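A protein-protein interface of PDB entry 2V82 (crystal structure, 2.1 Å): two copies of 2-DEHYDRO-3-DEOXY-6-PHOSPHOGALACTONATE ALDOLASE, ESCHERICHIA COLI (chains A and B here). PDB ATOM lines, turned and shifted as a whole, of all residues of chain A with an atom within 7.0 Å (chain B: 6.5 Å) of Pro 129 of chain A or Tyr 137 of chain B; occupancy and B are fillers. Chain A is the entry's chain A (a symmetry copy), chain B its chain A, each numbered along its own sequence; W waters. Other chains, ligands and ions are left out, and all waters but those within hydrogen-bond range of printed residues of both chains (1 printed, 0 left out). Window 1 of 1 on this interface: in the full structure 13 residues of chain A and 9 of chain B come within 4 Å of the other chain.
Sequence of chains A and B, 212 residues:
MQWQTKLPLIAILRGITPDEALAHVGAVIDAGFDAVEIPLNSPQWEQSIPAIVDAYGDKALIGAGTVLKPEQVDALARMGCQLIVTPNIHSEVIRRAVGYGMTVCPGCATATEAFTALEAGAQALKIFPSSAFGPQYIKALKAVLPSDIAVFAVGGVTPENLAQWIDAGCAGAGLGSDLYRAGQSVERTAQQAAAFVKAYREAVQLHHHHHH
Among the printed residues, merely in contact across the chains: Pro 87 of chain A with Ala 111 of chain B, Pro 129 of chain A with Tyr 137 of chain B, Ala 132 of chain A with Tyr 137 of chain B, Pro 129 of chain A with Ala 140 of chain B, Phe 128 of chain A with Ala 140 of chain B, Ala 109 of chain A with Thr 110 of chain B and Ala 132 of chain A with Phe 133 of chain B.
Hydrophobic or aromatic side chains of chain A that line the printed part of chain B: Ala 109, Phe 128, Pro 129 and Ala 132. Among the printed residues, 7 pairs touch across the chains. Among the printed residues, no Asp or Glu carboxylate lies within 4 Å of a Lys or Arg side-chain nitrogen of the other chain.
The side-chain hydroxyl (OH) of Tyr 137 of chain B sits at hydrogen-bond distance from the backbone carbonyl oxygen (O) of Ala 109 of chain B (2.4 Å). The backbone carbonyl oxygen of Cys 108 of chain A is in hydrogen-bond range of the backbone NH of Phe 128 of chain A (3.1 Å). The backbone carbonyl oxygen (O) of Ala 109 of chain A is in hydrogen-bond range of the side-chain hydroxyl (OH) of Tyr 137 of chain A (2.4 Å).
Water W1 lies within hydrogen-bond range of the side-chain hydroxyl of Tyr 137 of chain B, the backbone NH of Ala 111 of chain B and the backbone carbonyl oxygen of Phe 128 of chain A.
7 positions are printed for both chains.
Printed residues of chain B within 4 Å of Phe 128 of chain A: Ala 140. Pro 129 of chain A touches just these residues of chain B: Tyr 137 and Ala 140. Printed residues of chain B within 4 Å of Ala 132 of chain A: Phe 133 and Tyr 137. Phe 133 of chain A touches none of the printed residues of chain B. Of the printed residues of chain A, Tyr 137 of chain B touches Pro 129 (3.3 Å) and Ala 132 (3.3 Å). The nearest residue of chain B that does not touch Pro 129 of chain A is Leu 141 of chain B (4.9 Å). The nearest printed residue of chain A that does not touch Tyr 137 of chain B is Phe 133 of chain A (4.001 Å).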
ATOM      1  N   PRO A  87      22.952 -24.115 -19.363  1.00  0.00           N
ATOM      2  CA  PRO A  87      23.247 -25.049 -20.455  1.00  0.00           C
ATOM      3  C   PRO A  87      22.404 -26.320 -20.383  1.00  0.00           C
ATOM      4  O   PRO A  87      22.332 -27.077 -21.354  1.00  0.00           O
ATOM      5  CB  PRO A  87      24.722 -25.386 -20.246  1.00  0.00           C
ATOM      6  CG  PRO A  87      25.031 -25.043 -18.797  1.00  0.00           C
ATOM      7  CD  PRO A  87      23.869 -24.276 -18.216  1.00  0.00           C
ATOM      8  N   CYS A 108      18.124 -27.099 -23.223  1.00  0.00           N
ATOM      9  CA  CYS A 108      17.745 -28.477 -23.437  1.00  0.00           C
ATOM     10  C   CYS A 108      18.230 -28.875 -24.823  1.00  0.00           C
ATOM     11  O   CYS A 108      18.630 -28.025 -25.628  1.00  0.00           O
ATOM     12  CB  CYS A 108      16.238 -28.608 -23.325  1.00  0.00           C
ATOM     13  SG  CYS A 108      15.353 -27.538 -24.465  1.00  0.00           S
ATOM     14  N   ALA A 109      18.227 -30.168 -25.109  1.00  0.00           N
ATOM     15  CA  ALA A 109      18.717 -30.608 -26.403  1.00  0.00           C
ATOM     16  C   ALA A 109      17.805 -31.656 -27.040  1.00  0.00           C
ATOM     17  O   ALA A 109      18.006 -32.044 -28.205  1.00  0.00           O
ATOM     18  CB  ALA A 109      20.132 -31.121 -26.268  1.00  0.00           C
ATOM     19  N   LYS A 126      16.097 -22.706 -24.545  1.00  0.00           N
ATOM     20  CA  LYS A 126      17.357 -22.550 -25.260  1.00  0.00           C
ATOM     21  C   LYS A 126      17.663 -23.935 -25.822  1.00  0.00           C
ATOM     22  O   LYS A 126      17.652 -24.908 -25.085  1.00  0.00           O
ATOM     23  CB  LYS A 126      18.455 -22.050 -24.278  1.00  0.00           C
ATOM     24  CG  LYS A 126      19.936 -22.140 -24.727  1.00  0.00           C
ATOM     25  CD  LYS A 126      20.898 -22.141 -23.514  1.00  0.00           C
ATOM     26  CE  LYS A 126      22.428 -22.225 -23.829  1.00  0.00           C
ATOM     27  NZ  LYS A 126      23.219 -21.726 -22.607  1.00  0.00           N
ATOM     28  N   ILE A 127      17.908 -24.046 -27.123  1.00  0.00           N
ATOM     29  CA  ILE A 127      18.391 -25.313 -27.669  1.00  0.00           C
ATOM     30  C   ILE A 127      19.908 -25.202 -27.730  1.00  0.00           C
ATOM     31  O   ILE A 127      20.467 -24.355 -28.437  1.00  0.00           O
ATOM     32  CB  ILE A 127      17.749 -25.688 -29.054  1.00  0.00           C
ATOM     33  CG1 ILE A 127      16.210 -25.584 -29.013  1.00  0.00           C
ATOM     34  CG2 ILE A 127      18.184 -27.086 -29.516  1.00  0.00           C
ATOM     35  CD1 ILE A 127      15.505 -26.452 -27.956  1.00  0.00           C
ATOM     36  N   PHE A 128      20.579 -26.028 -26.951  1.00  0.00           N
ATOM     37  CA  PHE A 128      22.014 -25.922 -26.843  1.00  0.00           C
ATOM     38  C   PHE A 128      22.724 -27.277 -26.866  1.00  0.00           C
ATOM     39  O   PHE A 128      22.315 -28.199 -26.163  1.00  0.00           O
ATOM     40  CB  PHE A 128      22.388 -25.137 -25.578  1.00  0.00           C
ATOM     41  CG  PHE A 128      23.814 -25.271 -25.205  1.00  0.00           C
ATOM     42  CD1 PHE A 128      24.792 -24.552 -25.892  1.00  0.00           C
ATOM     43  CD2 PHE A 128      24.194 -26.139 -24.180  1.00  0.00           C
ATOM     44  CE1 PHE A 128      26.134 -24.711 -25.563  1.00  0.00           C
ATOM     45  CE2 PHE A 128      25.538 -26.298 -23.846  1.00  0.00           C
ATOM     46  CZ  PHE A 128      26.504 -25.584 -24.520  1.00  0.00           C
ATOM     47  N   PRO A 129      23.787 -27.395 -27.686  1.00  0.00           N
ATOM     48  CA  PRO A 129      24.200 -26.491 -28.768  1.00  0.00           C
ATOM     49  C   PRO A 129      23.435 -26.742 -30.070  1.00  0.00           C
ATOM     50  O   PRO A 129      23.369 -27.875 -30.554  1.00  0.00           O
ATOM     51  CB  PRO A 129      25.695 -26.808 -28.950  1.00  0.00           C
ATOM     52  CG  PRO A 129      26.051 -27.801 -27.847  1.00  0.00           C
ATOM     53  CD  PRO A 129      24.765 -28.470 -27.487  1.00  0.00           C
ATOM     54  N   SER A 130      22.860 -25.683 -30.625  1.00  0.00           N
ATOM     55  CA  SER A 130      21.993 -25.783 -31.807  1.00  0.00           C
ATOM     56  C   SER A 130      22.725 -26.249 -33.066  1.00  0.00           C
ATOM     57  O   SER A 130      22.121 -26.856 -33.946  1.00  0.00           O
ATOM     58  CB  SER A 130      21.361 -24.424 -32.077  1.00  0.00           C
ATOM     59  OG  SER A 130      20.506 -24.041 -31.021  1.00  0.00           O
ATOM     60  N   SER A 131      24.020 -25.934 -33.147  1.00  0.00           N
ATOM     61  CA  SER A 131      24.862 -26.186 -34.334  1.00  0.00           C
ATOM     62  C   SER A 131      24.935 -27.637 -34.787  1.00  0.00           C
ATOM     63  O   SER A 131      24.996 -27.925 -35.982  1.00  0.00           O
ATOM     64  CB  SER A 131      26.288 -25.697 -34.073  1.00  0.00           C
ATOM     65  OG  SER A 131      26.368 -24.297 -34.230  1.00  0.00           O
ATOM     66  N   ALA A 132      24.975 -28.542 -33.815  1.00  0.00           N
ATOM     67  CA  ALA A 132      25.011 -29.973 -34.076  1.00  0.00           C
ATOM     68  C   ALA A 132      23.698 -30.436 -34.685  1.00  0.00           C
ATOM     69  O   ALA A 132      23.686 -31.329 -35.538  1.00  0.00           O
ATOM     70  CB  ALA A 132      25.286 -30.731 -32.776  1.00  0.00           C
ATOM     71  N   PHE A 133      22.599 -29.816 -34.251  1.00  0.00           N
ATOM     72  CA  PHE A 133      21.261 -30.256 -34.638  1.00  0.00           C
ATOM     73  C   PHE A 133      20.783 -29.582 -35.915  1.00  0.00           C
ATOM     74  O   PHE A 133      20.263 -30.246 -36.808  1.00  0.00           O
ATOM     75  CB  PHE A 133      20.251 -30.010 -33.512  1.00  0.00           C
ATOM     76  CG  PHE A 133      20.660 -30.580 -32.178  1.00  0.00           C
ATOM     77  CD1 PHE A 133      20.706 -31.957 -31.975  1.00  0.00           C
ATOM     78  CD2 PHE A 133      20.987 -29.738 -31.124  1.00  0.00           C
ATOM     79  CE1 PHE A 133      21.079 -32.483 -30.748  1.00  0.00           C
ATOM     80  CE2 PHE A 133      21.366 -30.256 -29.889  1.00  0.00           C
ATOM     81  CZ  PHE A 133      21.422 -31.632 -29.705  1.00  0.00           C
ATOM     82  N   GLY A 134      20.958 -28.267 -36.005  1.00  0.00           N
ATOM     83  CA  GLY A 134      20.512 -27.516 -37.173  1.00  0.00           C
ATOM     84  C   GLY A 134      19.123 -26.910 -37.027  1.00  0.00           C
ATOM     85  O   GLY A 134      18.365 -27.293 -36.138  1.00  0.00           O
ATOM     86  N   TYR A 137      16.042 -29.152 -36.751  1.00  0.00           N
ATOM     87  CA  TYR A 137      15.802 -29.774 -35.453  1.00  0.00           C
ATOM     88  C   TYR A 137      14.744 -28.992 -34.697  1.00  0.00           C
ATOM     89  O   TYR A 137      13.781 -29.559 -34.189  1.00  0.00           O
ATOM     90  CB  TYR A 137      17.086 -29.819 -34.642  1.00  0.00           C
ATOM     91  CG  TYR A 137      17.030 -30.722 -33.436  1.00  0.00           C
ATOM     92  CD1 TYR A 137      16.961 -32.108 -33.582  1.00  0.00           C
ATOM     93  CD2 TYR A 137      17.088 -30.198 -32.148  1.00  0.00           C
ATOM     94  CE1 TYR A 137      16.938 -32.946 -32.460  1.00  0.00           C
ATOM     95  CE2 TYR A 137      17.057 -31.018 -31.033  1.00  0.00           C
ATOM     96  CZ  TYR A 137      16.974 -32.388 -31.191  1.00  0.00           C
ATOM     97  OH  TYR A 137      16.957 -33.202 -30.089  1.00  0.00           O
ATOM     98  N   ALA A 153      17.861 -20.414 -30.406  1.00  0.00           N
ATOM     99  CA  ALA A 153      19.061 -21.133 -30.838  1.00  0.00           C
ATOM    100  C   ALA A 153      20.293 -20.570 -30.121  1.00  0.00           C
ATOM    101  O   ALA A 153      20.481 -19.357 -30.058  1.00  0.00           O
ATOM    102  CB  ALA A 153      19.224 -21.029 -32.356  1.00  0.00           C
ATOM    103  N   VAL A 154      21.104 -21.445 -29.540  1.00  0.00           N
ATOM    104  CA  VAL A 154      22.383 -21.054 -28.932  1.00  0.00           C
ATOM    105  C   VAL A 154      23.414 -22.120 -29.284  1.00  0.00           C
ATOM    106  O   VAL A 154      23.212 -23.307 -29.008  1.00  0.00           O
ATOM    107  CB  VAL A 154      22.330 -20.947 -27.395  1.00  0.00           C
ATOM    108  CG1 VAL A 154      23.742 -20.658 -26.846  1.00  0.00           C
ATOM    109  CG2 VAL A 154      21.369 -19.869 -26.940  1.00  0.00           C
ATOM    110  N   GLY A 155      24.495 -21.693 -29.925  1.00  0.00           N
ATOM    111  CA  GLY A 155      25.609 -22.576 -30.250  1.00  0.00           C
ATOM    112  C   GLY A 155      25.851 -22.559 -31.729  1.00  0.00           C
ATOM    113  O   GLY A 155      25.055 -23.099 -32.486  1.00  0.00           O
ATOM    114  N   GLY A 156      26.944 -21.919 -32.144  1.00  0.00           N
ATOM    115  CA  GLY A 156      27.272 -21.781 -33.571  1.00  0.00           C
ATOM    116  C   GLY A 156      26.292 -20.963 -34.417  1.00  0.00           C
ATOM    117  O   GLY A 156      26.115 -21.239 -35.617  1.00  0.00           O
ATOM    118  N   TRP A 165      17.805 -19.722 -38.640  1.00  0.00           N
ATOM    119  CA  TRP A 165      17.253 -20.061 -37.335  1.00  0.00           C
ATOM    120  C   TRP A 165      15.877 -19.413 -37.151  1.00  0.00           C
ATOM    121  O   TRP A 165      14.927 -20.062 -36.695  1.00  0.00           O
ATOM    122  CB  TRP A 165      18.219 -19.663 -36.214  1.00  0.00           C
ATOM    123  CG  TRP A 165      19.569 -20.316 -36.368  1.00  0.00           C
ATOM    124  CD1 TRP A 165      20.693 -19.756 -36.918  1.00  0.00           C
ATOM    125  CD2 TRP A 165      19.921 -21.659 -36.018  1.00  0.00           C
ATOM    126  NE1 TRP A 165      21.728 -20.662 -36.908  1.00  0.00           N
ATOM    127  CE2 TRP A 165      21.280 -21.839 -36.364  1.00  0.00           C
ATOM    128  CE3 TRP A 165      19.221 -22.730 -35.448  1.00  0.00           C
ATOM    129  CZ2 TRP A 165      21.954 -23.043 -36.151  1.00  0.00           C
ATOM    130  CZ3 TRP A 165      19.894 -23.924 -35.229  1.00  0.00           C
ATOM    131  CH2 TRP A 165      21.246 -24.072 -35.585  1.00  0.00           C
ATOM    132  N   CYS B 108      26.966 -39.938 -22.128  1.00  0.00           N
ATOM    133  CA  CYS B 108      25.936 -38.924 -22.157  1.00  0.00           C
ATOM    134  C   CYS B 108      25.916 -38.330 -23.557  1.00  0.00           C
ATOM    135  O   CYS B 108      26.827 -38.565 -24.362  1.00  0.00           O
ATOM    136  CB  CYS B 108      26.243 -37.864 -21.117  1.00  0.00           C
ATOM    137  SG  CYS B 108      27.859 -37.110 -21.337  1.00  0.00           S
ATOM    138  N   ALA B 109      24.871 -37.582 -23.876  1.00  0.00           N
ATOM    139  CA  ALA B 109      24.781 -37.024 -25.213  1.00  0.00           C
ATOM    140  C   ALA B 109      24.354 -35.556 -25.198  1.00  0.00           C
ATOM    141  O   ALA B 109      24.355 -34.887 -26.247  1.00  0.00           O
ATOM    142  CB  ALA B 109      23.846 -37.858 -26.055  1.00  0.00           C
ATOM    143  N   THR B 110      23.985 -35.056 -24.021  1.00  0.00           N
ATOM    144  CA  THR B 110      23.504 -33.685 -23.886  1.00  0.00           C
ATOM    145  C   THR B 110      24.157 -33.036 -22.671  1.00  0.00           C
ATOM    146  O   THR B 110      24.690 -33.733 -21.806  1.00  0.00           O
ATOM    147  CB  THR B 110      21.963 -33.587 -23.699  1.00  0.00           C
ATOM    148  OG1 THR B 110      21.612 -34.027 -22.387  1.00  0.00           O
ATOM    149  CG2 THR B 110      21.173 -34.388 -24.744  1.00  0.00           C
ATOM    150  N   ALA B 111      24.102 -31.700 -22.604  1.00  0.00           N
ATOM    151  CA  ALA B 111      24.566 -30.983 -21.422  1.00  0.00           C
ATOM    152  C   ALA B 111      23.899 -31.486 -20.150  1.00  0.00           C
ATOM    153  O   ALA B 111      24.589 -31.809 -19.180  1.00  0.00           O
ATOM    154  CB  ALA B 111      24.376 -29.480 -21.577  1.00  0.00           C
ATOM    155  N   ILE B 127      31.094 -39.063 -24.732  1.00  0.00           N
ATOM    156  CA  ILE B 127      30.013 -38.527 -25.557  1.00  0.00           C
ATOM    157  C   ILE B 127      29.667 -39.613 -26.566  1.00  0.00           C
ATOM    158  O   ILE B 127      30.491 -40.010 -27.398  1.00  0.00           O
ATOM    159  CB  ILE B 127      30.359 -37.152 -26.234  1.00  0.00           C
ATOM    160  CG1 ILE B 127      30.910 -36.138 -25.209  1.00  0.00           C
ATOM    161  CG2 ILE B 127      29.148 -36.568 -26.975  1.00  0.00           C
ATOM    162  CD1 ILE B 127      29.989 -35.818 -24.018  1.00  0.00           C
ATOM    163  N   SER B 130      29.342 -39.899 -30.706  1.00  0.00           N
ATOM    164  CA  SER B 130      29.930 -38.601 -31.062  1.00  0.00           C
ATOM    165  C   SER B 130      29.731 -38.220 -32.529  1.00  0.00           C
ATOM    166  O   SER B 130      29.684 -37.039 -32.862  1.00  0.00           O
ATOM    167  CB  SER B 130      31.423 -38.632 -30.757  1.00  0.00           C
ATOM    168  OG  SER B 130      31.656 -38.778 -29.374  1.00  0.00           O
ATOM    169  N   PHE B 133      27.021 -35.856 -33.633  1.00  0.00           N
ATOM    170  CA  PHE B 133      27.176 -34.502 -33.107  1.00  0.00           C
ATOM    171  C   PHE B 133      28.366 -33.781 -33.724  1.00  0.00           C
ATOM    172  O   PHE B 133      28.248 -32.625 -34.125  1.00  0.00           O
ATOM    173  CB  PHE B 133      27.313 -34.515 -31.581  1.00  0.00           C
ATOM    174  CG  PHE B 133      26.219 -35.268 -30.868  1.00  0.00           C
ATOM    175  CD1 PHE B 133      24.914 -34.781 -30.849  1.00  0.00           C
ATOM    176  CD2 PHE B 133      26.497 -36.455 -30.205  1.00  0.00           C
ATOM    177  CE1 PHE B 133      23.906 -35.469 -30.192  1.00  0.00           C
ATOM    178  CE2 PHE B 133      25.493 -37.157 -29.545  1.00  0.00           C
ATOM    179  CZ  PHE B 133      24.193 -36.666 -29.548  1.00  0.00           C
ATOM    180  N   GLY B 134      29.507 -34.456 -33.802  1.00  0.00           N
ATOM    181  CA  GLY B 134      30.716 -33.852 -34.350  1.00  0.00           C
ATOM    182  C   GLY B 134      31.628 -33.230 -33.302  1.00  0.00           C
ATOM    183  O   GLY B 134      31.212 -33.004 -32.167  1.00  0.00           O
ATOM    184  N   PRO B 135      32.885 -32.935 -33.688  1.00  0.00           N
ATOM    185  CA  PRO B 135      33.890 -32.331 -32.809  1.00  0.00           C
ATOM    186  C   PRO B 135      33.407 -31.038 -32.175  1.00  0.00           C
ATOM    187  O   PRO B 135      33.682 -30.793 -31.005  1.00  0.00           O
ATOM    188  CB  PRO B 135      35.056 -32.050 -33.762  1.00  0.00           C
ATOM    189  CG  PRO B 135      34.895 -33.068 -34.824  1.00  0.00           C
ATOM    190  CD  PRO B 135      33.424 -33.180 -35.036  1.00  0.00           C
ATOM    191  N   GLN B 136      32.677 -30.237 -32.956  1.00  0.00           N
ATOM    192  CA  GLN B 136      32.172 -28.931 -32.527  1.00  0.00           C
ATOM    193  C   GLN B 136      31.201 -29.056 -31.358  1.00  0.00           C
ATOM    194  O   GLN B 136      31.108 -28.152 -30.529  1.00  0.00           O
ATOM    195  CB  GLN B 136      31.506 -28.194 -33.700  1.00  0.00           C
ATOM    196  CG  GLN B 136      30.955 -26.809 -33.360  1.00  0.00           C
ATOM    197  CD  GLN B 136      32.049 -25.805 -33.002  1.00  0.00           C
ATOM    198  OE1 GLN B 136      33.085 -25.709 -33.692  1.00  0.00           O
ATOM    199  NE2 GLN B 136      31.822 -25.044 -31.919  1.00  0.00           N
ATOM    200  N   TYR B 137      30.492 -30.184 -31.294  1.00  0.00           N
ATOM    201  CA  TYR B 137      29.563 -30.436 -30.197  1.00  0.00           C
ATOM    202  C   TYR B 137      30.317 -30.460 -28.880  1.00  0.00           C
ATOM    203  O   TYR B 137      29.934 -29.798 -27.920  1.00  0.00           O
ATOM    204  CB  TYR B 137      28.848 -31.760 -30.403  1.00  0.00           C
ATOM    205  CG  TYR B 137      27.645 -31.963 -29.516  1.00  0.00           C
ATOM    206  CD1 TYR B 137      26.489 -31.202 -29.691  1.00  0.00           C
ATOM    207  CD2 TYR B 137      27.643 -32.944 -28.528  1.00  0.00           C
ATOM    208  CE1 TYR B 137      25.363 -31.412 -28.886  1.00  0.00           C
ATOM    209  CE2 TYR B 137      26.539 -33.151 -27.720  1.00  0.00           C
ATOM    210  CZ  TYR B 137      25.405 -32.381 -27.895  1.00  0.00           C
ATOM    211  OH  TYR B 137      24.306 -32.595 -27.105  1.00  0.00           O
ATOM    212  N   ILE B 138      31.393 -31.231 -28.858  1.00  0.00           N
ATOM    213  CA  ILE B 138      32.260 -31.340 -27.696  1.00  0.00           C
ATOM    214  C   ILE B 138      32.867 -29.976 -27.346  1.00  0.00           C
ATOM    215  O   ILE B 138      32.833 -29.575 -26.192  1.00  0.00           O
ATOM    216  CB  ILE B 138      33.325 -32.463 -27.911  1.00  0.00           C
ATOM    217  CG1 ILE B 138      32.655 -33.828 -27.727  1.00  0.00           C
ATOM    218  CG2 ILE B 138      34.505 -32.339 -26.954  1.00  0.00           C
ATOM    219  CD1 ILE B 138      33.097 -34.875 -28.710  1.00  0.00           C
ATOM    220  N   LYS B 139      33.395 -29.264 -28.340  1.00  0.00           N
ATOM    221  CA  LYS B 139      33.927 -27.910 -28.139  1.00  0.00           C
ATOM    222  C   LYS B 139      32.883 -27.037 -27.433  1.00  0.00           C
ATOM    223  O   LYS B 139      33.198 -26.286 -26.500  1.00  0.00           O
ATOM    224  CB  LYS B 139      34.312 -27.308 -29.490  1.00  0.00           C
ATOM    225  CG  LYS B 139      35.303 -26.160 -29.458  1.00  0.00           C
ATOM    226  CD  LYS B 139      35.902 -25.947 -30.864  1.00  0.00           C
ATOM    227  CE  LYS B 139      36.026 -24.461 -31.232  1.00  0.00           C
ATOM    228  NZ  LYS B 139      36.319 -24.269 -32.702  1.00  0.00           N
ATOM    229  N   ALA B 140      31.633 -27.142 -27.880  1.00  0.00           N
ATOM    230  CA  ALA B 140      30.552 -26.386 -27.257  1.00  0.00           C
ATOM    231  C   ALA B 140      30.275 -26.882 -25.826  1.00  0.00           C
ATOM    232  O   ALA B 140      30.033 -26.083 -24.921  1.00  0.00           O
ATOM    233  CB  ALA B 140      29.295 -26.433 -28.125  1.00  0.00           C
ATOM    234  N   LEU B 141      30.363 -28.192 -25.607  1.00  0.00           N
ATOM    235  CA  LEU B 141      30.138 -28.725 -24.267  1.00  0.00           C
ATOM    236  C   LEU B 141      31.245 -28.319 -23.309  1.00  0.00           C
ATOM    237  O   LEU B 141      30.978 -27.961 -22.145  1.00  0.00           O
ATOM    238  CB  LEU B 141      29.935 -30.236 -24.281  1.00  0.00           C
ATOM    239  CG  LEU B 141      28.548 -30.715 -24.714  1.00  0.00           C
ATOM    240  CD1 LEU B 141      28.542 -32.209 -24.790  1.00  0.00           C
ATOM    241  CD2 LEU B 141      27.484 -30.240 -23.719  1.00  0.00           C
ATOM    242  N   LYS B 142      32.476 -28.310 -23.820  1.00  0.00           N
ATOM    243  CA  LYS B 142      33.646 -27.914 -23.033  1.00  0.00           C
ATOM    244  C   LYS B 142      33.588 -26.462 -22.549  1.00  0.00           C
ATOM    245  O   LYS B 142      34.282 -26.083 -21.602  1.00  0.00           O
ATOM    246  CB  LYS B 142      34.931 -28.163 -23.829  1.00  0.00           C
ATOM    247  CG  LYS B 142      35.142 -29.629 -24.265  1.00  0.00           C
ATOM    248  CD  LYS B 142      35.726 -30.509 -23.169  1.00  0.00           C
ATOM    249  CE  LYS B 142      37.069 -29.969 -22.680  1.00  0.00           C
ATOM    250  NZ  LYS B 142      37.623 -30.821 -21.585  1.00  0.00           N
ATOM    251  N   ALA B 168      39.309 -30.509 -30.913  1.00  0.00           N
ATOM    252  CA  ALA B 168      38.055 -30.008 -30.362  1.00  0.00           C
ATOM    253  C   ALA B 168      38.000 -30.002 -28.828  1.00  0.00           C
ATOM    254  O   ALA B 168      37.147 -29.326 -28.237  1.00  0.00           O
ATOM    255  CB  ALA B 168      36.905 -30.813 -30.909  1.00  0.00           C
HETATM  256  O   HOH W   1      23.507 -30.771 -25.201  1.00  0.00           O
